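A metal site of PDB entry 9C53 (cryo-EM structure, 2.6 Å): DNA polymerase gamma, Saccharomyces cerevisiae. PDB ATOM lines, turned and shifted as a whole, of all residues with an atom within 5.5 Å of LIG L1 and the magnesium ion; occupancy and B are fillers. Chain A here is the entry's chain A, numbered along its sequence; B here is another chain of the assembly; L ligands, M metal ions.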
ATOM      1  N   ARG A 629      -2.000 -13.607  13.698  1.00  0.00           N
ATOM      2  CA  ARG A 629      -2.847 -14.679  13.204  1.00  0.00           C
ATOM      3  C   ARG A 629      -3.587 -15.337  14.358  1.00  0.00           C
ATOM      4  O   ARG A 629      -3.166 -15.260  15.511  1.00  0.00           O
ATOM      5  CB  ARG A 629      -2.039 -15.729  12.432  1.00  0.00           C
ATOM      6  CG  ARG A 629      -1.151 -15.157  11.339  1.00  0.00           C
ATOM      7  CD  ARG A 629      -1.145 -16.055  10.109  1.00  0.00           C
ATOM      8  NE  ARG A 629      -0.503 -17.343  10.370  1.00  0.00           N
ATOM      9  CZ  ARG A 629      -0.182 -18.214   9.431  1.00  0.00           C
ATOM     10  NH1 ARG A 629      -0.411 -17.980   8.147  1.00  0.00           N
ATOM     11  NH2 ARG A 629       0.377 -19.374   9.788  1.00  0.00           N
ATOM     12  N   ASP A 666     -11.512 -20.767  -1.220  1.00  0.00           N
ATOM     13  CA  ASP A 666     -10.098 -20.716  -0.756  1.00  0.00           C
ATOM     14  C   ASP A 666      -9.251 -19.896  -1.728  1.00  0.00           C
ATOM     15  O   ASP A 666      -9.474 -20.019  -2.948  1.00  0.00           O
ATOM     16  CB  ASP A 666      -9.512 -22.127  -0.613  1.00  0.00           C
ATOM     17  CG  ASP A 666      -8.255 -22.186   0.244  1.00  0.00           C
ATOM     18  OD1 ASP A 666      -7.159 -22.286  -0.330  1.00  0.00           O
ATOM     19  OD2 ASP A 666      -8.388 -22.150   1.480  1.00  0.00           O
ATOM     20  N   VAL A 667      -8.315 -19.091  -1.224  1.00  0.00           N
ATOM     21  CA  VAL A 667      -7.450 -18.210  -2.083  1.00  0.00           C
ATOM     22  C   VAL A 667      -6.423 -19.057  -2.834  1.00  0.00           C
ATOM     23  O   VAL A 667      -6.075 -20.141  -2.325  1.00  0.00           O
ATOM     24  CB  VAL A 667      -6.789 -17.082  -1.262  1.00  0.00           C
ATOM     25  CG1 VAL A 667      -6.214 -15.990  -2.149  1.00  0.00           C
ATOM     26  CG2 VAL A 667      -7.742 -16.497  -0.234  1.00  0.00           C
ATOM     27  N   ASP A 668      -5.941 -18.591  -3.989  1.00  0.00           N
ATOM     28  CA  ASP A 668      -4.994 -19.384  -4.824  1.00  0.00           C
ATOM     29  C   ASP A 668      -3.617 -18.714  -4.879  1.00  0.00           C
ATOM     30  O   ASP A 668      -3.567 -17.528  -5.234  1.00  0.00           O
ATOM     31  CB  ASP A 668      -5.561 -19.572  -6.229  1.00  0.00           C
ATOM     32  CG  ASP A 668      -7.014 -20.003  -6.244  1.00  0.00           C
ATOM     33  OD1 ASP A 668      -7.390 -20.831  -5.393  1.00  0.00           O
ATOM     34  OD2 ASP A 668      -7.766 -19.500  -7.102  1.00  0.00           O
ATOM     35  N   SER A 669      -2.549 -19.447  -4.529  1.00  0.00           N
ATOM     36  CA  SER A 669      -1.156 -18.914  -4.592  1.00  0.00           C
ATOM     37  C   SER A 669      -1.098 -17.570  -3.850  1.00  0.00           C
ATOM     38  O   SER A 669      -0.570 -16.616  -4.435  1.00  0.00           O
ATOM     39  CB  SER A 669      -0.689 -18.794  -6.013  1.00  0.00           C
ATOM     40  OG  SER A 669      -0.584 -20.081  -6.606  1.00  0.00           O
ATOM     41  N   GLU A 670      -1.608 -17.522  -2.624  1.00  0.00           N
ATOM     42  CA  GLU A 670      -1.732 -16.220  -1.901  1.00  0.00           C
ATOM     43  C   GLU A 670      -0.397 -15.529  -1.612  1.00  0.00           C
ATOM     44  O   GLU A 670      -0.309 -14.323  -1.896  1.00  0.00           O
ATOM     45  CB  GLU A 670      -2.452 -16.471  -0.570  1.00  0.00           C
ATOM     46  CG  GLU A 670      -2.979 -15.200   0.070  1.00  0.00           C
ATOM     47  CD  GLU A 670      -3.313 -15.349   1.548  1.00  0.00           C
ATOM     48  OE1 GLU A 670      -2.563 -16.045   2.248  1.00  0.00           O
ATOM     49  OE2 GLU A 670      -4.316 -14.763   1.986  1.00  0.00           O
ATOM     50  N   GLU A 671       0.624 -16.238  -1.128  1.00  0.00           N
ATOM     51  CA  GLU A 671       1.871 -15.535  -0.693  1.00  0.00           C
ATOM     52  C   GLU A 671       2.849 -15.388  -1.862  1.00  0.00           C
ATOM     53  O   GLU A 671       3.781 -14.591  -1.735  1.00  0.00           O
ATOM     54  CB  GLU A 671       2.487 -16.267   0.504  1.00  0.00           C
ATOM     55  CG  GLU A 671       1.947 -15.759   1.829  1.00  0.00           C
ATOM     56  CD  GLU A 671       2.601 -16.347   3.068  1.00  0.00           C
ATOM     57  OE1 GLU A 671       3.852 -16.341   3.140  1.00  0.00           O
ATOM     58  OE2 GLU A 671       1.863 -16.818   3.958  1.00  0.00           O
ATOM     59  N   LYS A 700      -5.029 -22.359 -12.853  1.00  0.00           N
ATOM     60  CA  LYS A 700      -5.113 -23.666 -12.226  1.00  0.00           C
ATOM     61  C   LYS A 700      -6.118 -24.573 -12.932  1.00  0.00           C
ATOM     62  O   LYS A 700      -5.926 -25.804 -12.978  1.00  0.00           O
ATOM     63  CB  LYS A 700      -5.472 -23.530 -10.743  1.00  0.00           C
ATOM     64  CG  LYS A 700      -5.238 -24.801  -9.946  1.00  0.00           C
ATOM     65  CD  LYS A 700      -5.886 -24.724  -8.575  1.00  0.00           C
ATOM     66  CE  LYS A 700      -5.128 -23.777  -7.664  1.00  0.00           C
ATOM     67  NZ  LYS A 700      -5.633 -23.826  -6.265  1.00  0.00           N
ATOM     68  N   HIS A 707       3.070 -24.082  -9.598  1.00  0.00           N
ATOM     69  CA  HIS A 707       3.298 -25.208  -8.704  1.00  0.00           C
ATOM     70  C   HIS A 707       3.189 -26.529  -9.458  1.00  0.00           C
ATOM     71  O   HIS A 707       3.989 -27.451  -9.226  1.00  0.00           O
ATOM     72  CB  HIS A 707       2.306 -25.170  -7.544  1.00  0.00           C
ATOM     73  CG  HIS A 707       2.649 -24.165  -6.482  1.00  0.00           C
ATOM     74  ND1 HIS A 707       3.918 -24.058  -5.954  1.00  0.00           N
ATOM     75  CD2 HIS A 707       1.895 -23.238  -5.851  1.00  0.00           C
ATOM     76  CE1 HIS A 707       3.930 -23.101  -5.046  1.00  0.00           C
ATOM     77  NE2 HIS A 707       2.717 -22.589  -4.967  1.00  0.00           N
ATOM     78  N   ARG A 718       1.928 -32.042  -5.863  1.00  0.00           N
ATOM     79  CA  ARG A 718       1.817 -30.578  -5.867  1.00  0.00           C
ATOM     80  C   ARG A 718       2.122 -29.995  -4.484  1.00  0.00           C
ATOM     81  O   ARG A 718       2.699 -28.899  -4.391  1.00  0.00           O
ATOM     82  CB  ARG A 718       0.422 -30.167  -6.331  1.00  0.00           C
ATOM     83  CG  ARG A 718       0.359 -28.791  -6.980  1.00  0.00           C
ATOM     84  CD  ARG A 718      -1.072 -28.333  -7.135  1.00  0.00           C
ATOM     85  NE  ARG A 718      -1.170 -26.908  -7.451  1.00  0.00           N
ATOM     86  CZ  ARG A 718      -1.701 -26.004  -6.644  1.00  0.00           C
ATOM     87  NH1 ARG A 718      -2.197 -26.324  -5.469  1.00  0.00           N
ATOM     88  NH2 ARG A 718      -1.728 -24.732  -7.038  1.00  0.00           N
ATOM     89  N   LYS A 722       4.914 -27.235  -3.452  1.00  0.00           N
ATOM     90  CA  LYS A 722       4.647 -26.028  -2.679  1.00  0.00           C
ATOM     91  C   LYS A 722       5.639 -25.888  -1.529  1.00  0.00           C
ATOM     92  O   LYS A 722       6.140 -24.792  -1.257  1.00  0.00           O
ATOM     93  CB  LYS A 722       3.220 -26.043  -2.140  1.00  0.00           C
ATOM     94  CG  LYS A 722       2.190 -25.487  -3.106  1.00  0.00           C
ATOM     95  CD  LYS A 722       0.857 -25.235  -2.408  1.00  0.00           C
ATOM     96  CE  LYS A 722       0.320 -26.486  -1.740  1.00  0.00           C
ATOM     97  NZ  LYS A 722      -0.930 -26.218  -0.988  1.00  0.00           N
ATOM     98  N   ILE A 723       5.943 -26.997  -0.853  1.00  0.00           N
ATOM     99  CA  ILE A 723       6.938 -26.984   0.231  1.00  0.00           C
ATOM    100  C   ILE A 723       8.305 -26.590  -0.313  1.00  0.00           C
ATOM    101  O   ILE A 723       9.013 -25.764   0.278  1.00  0.00           O
ATOM    102  CB  ILE A 723       6.980 -28.354   0.938  1.00  0.00           C
ATOM    103  CG1 ILE A 723       5.638 -28.659   1.608  1.00  0.00           C
ATOM    104  CG2 ILE A 723       8.109 -28.390   1.960  1.00  0.00           C
ATOM    105  CD1 ILE A 723       5.574 -30.024   2.231  1.00  0.00           C
ATOM    106  N   TYR A 726       8.255 -22.734  -1.211  1.00  0.00           N
ATOM    107  CA  TYR A 726       8.217 -21.843  -0.061  1.00  0.00           C
ATOM    108  C   TYR A 726       9.466 -21.952   0.796  1.00  0.00           C
ATOM    109  O   TYR A 726       9.836 -20.999   1.484  1.00  0.00           O
ATOM    110  CB  TYR A 726       6.964 -22.101   0.770  1.00  0.00           C
ATOM    111  CG  TYR A 726       5.704 -21.573   0.126  1.00  0.00           C
ATOM    112  CD1 TYR A 726       5.661 -20.301  -0.423  1.00  0.00           C
ATOM    113  CD2 TYR A 726       4.560 -22.352   0.061  1.00  0.00           C
ATOM    114  CE1 TYR A 726       4.515 -19.810  -1.021  1.00  0.00           C
ATOM    115  CE2 TYR A 726       3.402 -21.881  -0.531  1.00  0.00           C
ATOM    116  CZ  TYR A 726       3.395 -20.603  -1.069  1.00  0.00           C
ATOM    117  OH  TYR A 726       2.243 -20.125  -1.659  1.00  0.00           O
ATOM    118  N   GLY A 727      10.125 -23.112   0.774  1.00  0.00           N
ATOM    119  CA  GLY A 727      11.438 -23.204   1.406  1.00  0.00           C
ATOM    120  C   GLY A 727      12.492 -22.398   0.684  1.00  0.00           C
ATOM    121  O   GLY A 727      13.401 -21.855   1.325  1.00  0.00           O
ATOM    122  N   TYR A 730      12.131 -18.291   1.298  1.00  0.00           N
ATOM    123  CA  TYR A 730      12.863 -17.961   2.503  1.00  0.00           C
ATOM    124  C   TYR A 730      14.243 -18.621   2.458  1.00  0.00           C
ATOM    125  O   TYR A 730      14.590 -19.330   1.515  1.00  0.00           O
ATOM    126  CB  TYR A 730      12.068 -18.382   3.734  1.00  0.00           C
ATOM    127  CG  TYR A 730      10.635 -17.894   3.669  1.00  0.00           C
ATOM    128  CD1 TYR A 730      10.350 -16.551   3.433  1.00  0.00           C
ATOM    129  CD2 TYR A 730       9.574 -18.762   3.828  1.00  0.00           C
ATOM    130  CE1 TYR A 730       9.042 -16.098   3.360  1.00  0.00           C
ATOM    131  CE2 TYR A 730       8.266 -18.324   3.756  1.00  0.00           C
ATOM    132  CZ  TYR A 730       8.009 -16.981   3.527  1.00  0.00           C
ATOM    133  OH  TYR A 730       6.713 -16.537   3.451  1.00  0.00           O
ATOM    134  N   ASP A 865      -6.913 -18.199   5.019  1.00  0.00           N
ATOM    135  CA  ASP A 865      -7.042 -18.268   3.527  1.00  0.00           C
ATOM    136  C   ASP A 865      -8.331 -19.017   3.119  1.00  0.00           C
ATOM    137  O   ASP A 865      -8.587 -19.102   1.908  1.00  0.00           O
ATOM    138  CB  ASP A 865      -5.738 -18.776   2.892  1.00  0.00           C
ATOM    139  CG  ASP A 865      -5.863 -19.996   2.004  1.00  0.00           C
ATOM    140  OD1 ASP A 865      -5.864 -21.124   2.541  1.00  0.00           O
ATOM    141  OD2 ASP A 865      -5.937 -19.822   0.771  1.00  0.00           O
ATOM    142  P    DT B  18      17.874 -24.599   6.737  1.00  0.00           P
ATOM    143  OP1  DT B  18      17.627 -25.662   7.730  1.00  0.00           O
ATOM    144  OP2  DT B  18      18.652 -24.916   5.521  1.00  0.00           O
ATOM    145  O5'  DT B  18      16.478 -23.975   6.269  1.00  0.00           O
ATOM    146  C5'  DT B  18      15.495 -23.593   7.243  1.00  0.00           C
ATOM    147  C4'  DT B  18      14.616 -22.490   6.704  1.00  0.00           C
ATOM    148  O4'  DT B  18      13.849 -22.981   5.581  1.00  0.00           O
ATOM    149  C3'  DT B  18      13.564 -21.977   7.676  1.00  0.00           C
ATOM    150  O3'  DT B  18      14.126 -20.983   8.522  1.00  0.00           O
ATOM    151  C2'  DT B  18      12.520 -21.375   6.731  1.00  0.00           C
ATOM    152  C1'  DT B  18      12.605 -22.304   5.509  1.00  0.00           C
ATOM    153  N1   DT B  18      11.508 -23.313   5.457  1.00  0.00           N
ATOM    154  C2   DT B  18      10.246 -22.923   5.060  1.00  0.00           C
ATOM    155  O2   DT B  18       9.971 -21.780   4.749  1.00  0.00           O
ATOM    156  N3   DT B  18       9.318 -23.923   5.035  1.00  0.00           N
ATOM    157  C4   DT B  18       9.514 -25.246   5.366  1.00  0.00           C
ATOM    158  O4   DT B  18       8.612 -26.078   5.323  1.00  0.00           O
ATOM    159  C5   DT B  18      10.853 -25.595   5.773  1.00  0.00           C
ATOM    160  C7   DT B  18      11.185 -27.005   6.158  1.00  0.00           C
ATOM    161  C6   DT B  18      11.781 -24.623   5.801  1.00  0.00           C
ATOM    162  P    DA B  19      13.613 -20.822  10.033  1.00  0.00           P
ATOM    163  OP1  DA B  19      14.521 -19.877  10.717  1.00  0.00           O
ATOM    164  OP2  DA B  19      13.404 -22.171  10.593  1.00  0.00           O
ATOM    165  O5'  DA B  19      12.178 -20.128   9.891  1.00  0.00           O
ATOM    166  C5'  DA B  19      12.083 -18.748   9.547  1.00  0.00           C
ATOM    167  C4'  DA B  19      10.632 -18.334   9.371  1.00  0.00           C
ATOM    168  O4'  DA B  19      10.055 -19.040   8.260  1.00  0.00           O
ATOM    169  C3'  DA B  19       9.719 -18.668  10.548  1.00  0.00           C
ATOM    170  O3'  DA B  19       9.789 -17.637  11.521  1.00  0.00           O
ATOM    171  C2'  DA B  19       8.351 -18.713   9.885  1.00  0.00           C
ATOM    172  C1'  DA B  19       8.669 -19.224   8.473  1.00  0.00           C
ATOM    173  N9   DA B  19       8.338 -20.629   8.270  1.00  0.00           N
ATOM    174  C8   DA B  19       9.208 -21.654   8.068  1.00  0.00           C
ATOM    175  N7   DA B  19       8.619 -22.827   7.917  1.00  0.00           N
ATOM    176  C5   DA B  19       7.267 -22.532   8.029  1.00  0.00           C
ATOM    177  C6   DA B  19       6.123 -23.334   7.954  1.00  0.00           C
ATOM    178  N6   DA B  19       6.155 -24.658   7.741  1.00  0.00           N
ATOM    179  N1   DA B  19       4.928 -22.730   8.105  1.00  0.00           N
ATOM    180  C2   DA B  19       4.889 -21.412   8.315  1.00  0.00           C
ATOM    181  N3   DA B  19       5.899 -20.553   8.401  1.00  0.00           N
ATOM    182  C4   DA B  19       7.081 -21.185   8.245  1.00  0.00           C
HETATM  183  P1  LIG L   1      -3.318 -23.075  -3.131  1.00  0.00           P
HETATM  184  O1  LIG L   1      -3.280 -24.571  -2.979  1.00  0.00           O
HETATM  185  O2  LIG L   1      -4.383 -22.438  -2.282  1.00  0.00           O
HETATM  186  O3  LIG L   1      -3.383 -22.637  -4.563  1.00  0.00           O
HETATM  187  P2  LIG L   1      -1.459 -21.517  -1.424  1.00  0.00           P
HETATM  188  O4  LIG L   1      -2.575 -20.583  -1.131  1.00  0.00           O
HETATM  189  O5  LIG L   1      -0.114 -20.972  -1.761  1.00  0.00           O
HETATM  190  O6  LIG L   1      -1.903 -22.526  -2.589  1.00  0.00           O
HETATM  191  P3  LIG L   1      -2.225 -22.933   1.048  1.00  0.00           P
HETATM  192  O7  LIG L   1      -3.640 -23.004   0.598  1.00  0.00           O
HETATM  193  O8  LIG L   1      -1.643 -24.137   1.704  1.00  0.00           O
HETATM  194  O9  LIG L   1      -1.298 -22.536  -0.202  1.00  0.00           O
HETATM  195  O10 LIG L   1      -2.027 -21.662   1.989  1.00  0.00           O
HETATM  196  C1  LIG L   1      -1.055 -21.756   3.072  1.00  0.00           C
HETATM  197  C2  LIG L   1      -0.465 -20.395   3.331  1.00  0.00           C
HETATM  198  O11 LIG L   1       0.650 -20.528   4.225  1.00  0.00           O
HETATM  199  C3  LIG L   1       0.074 -19.685   2.084  1.00  0.00           C
HETATM  200  O12 LIG L   1      -0.013 -18.277   2.250  1.00  0.00           O
HETATM  201  C4  LIG L   1       1.527 -20.156   2.040  1.00  0.00           C
HETATM  202  C5  LIG L   1       1.871 -20.480   3.484  1.00  0.00           C
HETATM  203  N1  LIG L   1       2.545 -21.774   3.634  1.00  0.00           N
HETATM  204  C6  LIG L   1       1.988 -23.016   3.513  1.00  0.00           C
HETATM  205  N2  LIG L   1       2.860 -23.982   3.703  1.00  0.00           N
HETATM  206  C7  LIG L   1       4.058 -23.330   3.943  1.00  0.00           C
HETATM  207  C8  LIG L   1       5.359 -23.784   4.217  1.00  0.00           C
HETATM  208  N3  LIG L   1       5.690 -25.075   4.283  1.00  0.00           N
HETATM  209  N4  LIG L   1       6.317 -22.860   4.418  1.00  0.00           N
HETATM  210  C9  LIG L   1       5.981 -21.562   4.347  1.00  0.00           C
HETATM  211  N5  LIG L   1       4.796 -21.012   4.101  1.00  0.00           N
HETATM  212  C10 LIG L   1       3.866 -21.965   3.911  1.00  0.00           C
HETATM  213  P1  LG2 L   2      -4.079 -27.016   5.060  1.00  0.00           P
HETATM  214  O1  LG2 L   2      -5.521 -27.218   5.420  1.00  0.00           O
HETATM  215  O2  LG2 L   2      -3.320 -28.293   5.349  1.00  0.00           O
HETATM  216  O3  LG2 L   2      -3.468 -25.798   5.969  1.00  0.00           O
HETATM  217  N1  LG2 L   2      -0.479 -23.879   7.450  1.00  0.00           N
HETATM  218  C1  LG2 L   2      -0.511 -25.286   7.169  1.00  0.00           C
HETATM  219  C2  LG2 L   2       0.810 -23.137   7.436  1.00  0.00           C
HETATM  220  O4  LG2 L   2       0.839 -21.976   7.675  1.00  0.00           O
HETATM  221  N2  LG2 L   2       2.076 -23.859   7.130  1.00  0.00           N
HETATM  222  C3  LG2 L   2       2.042 -25.288   6.839  1.00  0.00           C
HETATM  223  O5  LG2 L   2       3.046 -25.862   6.592  1.00  0.00           O
HETATM  224  C4  LG2 L   2       0.736 -26.015   6.852  1.00  0.00           C
HETATM  225  C5  LG2 L   2       0.699 -27.508   6.555  1.00  0.00           C
HETATM  226  C6  LG2 L   2      -2.263 -22.391   6.450  1.00  0.00           C
HETATM  227  C7  LG2 L   2      -4.351 -25.075   6.772  1.00  0.00           C
HETATM  228  C8  LG2 L   2      -3.805 -23.831   7.126  1.00  0.00           C
HETATM  229  O6  LG2 L   2      -2.621 -24.015   8.121  1.00  0.00           O
HETATM  230  C9  LG2 L   2      -1.711 -23.173   7.756  1.00  0.00           C
HETATM  231  C10 LG2 L   2      -3.174 -23.136   5.919  1.00  0.00           C
HETATM  232 MG    MG M   1      -5.046 -20.983  -0.790  1.00  0.00          MG
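O3 of LIG L1 is in salt-bridge range of NZ of Lys 700, at 3.1 Å.
An oxygen (O8) of LIG L1 is in salt-bridge range of the side-chain amino group (NZ) of Lys 722 (3.5 Å).
An oxygen (O1) of LIG L1 lies within salt-bridge range of the guanidinium group (NH1) of Arg 718 (3.2 Å).
The guanidinium group (NH2) of Arg 629 is in hydrogen-bond range of an oxygen (O4) of LG2 L2.
OH of Tyr 726 is in hydrogen-bond range of O5 of LIG L1 (2.5 Å).
An oxygen (O3) of LIG L1 is in hydrogen-bond range of the backbone NH (N) of Ser 669, at 3.3 Å.
An oxygen (O12) of LIG L1 is in hydrogen-bond range of the side-chain carboxylate (OE2) of Glu 671.
O4 of DT 18 of chain B lies within hydrogen-bond range of a nitrogen (N3) of LIG L1 (3.3 Å).
N1 of DA 19 of chain B lies within hydrogen-bond range of N2 of LG2 L2 (3.2 Å).
OE1 of Glu 670 lies within hydrogen-bond range of O12 of LIG L1 (3.4 Å).
OD1 of Asp 668 lies within salt-bridge range of NZ of Lys 700 (3.6 Å).
The side-chain hydroxyl (OH) of Tyr 730 lies within hydrogen-bond range of the side-chain carboxylate (OE1) of Glu 671.
Asp 668 touches LIG L1 (CA to O3, 3.6 Å).
DA 19 of chain B touches LIG L1 (N6 to N3, 3.5 Å).
Hydrophobic or aromatic side chains within 4 Å of LIG L1: Tyr 726.
Within 4 Å of LIG L1: Asp 666, Val 667, Asp 668, Ser 669, Glu 670, Glu 671, Lys 700, Arg 718, Lys 722, Tyr 726, Asp 865, DT 18 of chain B and DA 19 of chain B.
Within 4 Å of the magnesium ion: Asp 666, Val 667 and Asp 865.
The nearest printed residue that does not touch the magnesium ion is Asp 668 (4.1 Å).
The magnesium ion is bound by O of Val 667 (2.0 Å), OD2 of Asp 865 (2.1 Å), O2 of LIG L1 (2.2 Å), OD1 of Asp 666 (2.5 Å) and O4 of LIG L1 (2.5 Å).
Slightly farther from the magnesium ion lies O7 of LIG L1 (2.8 Å).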
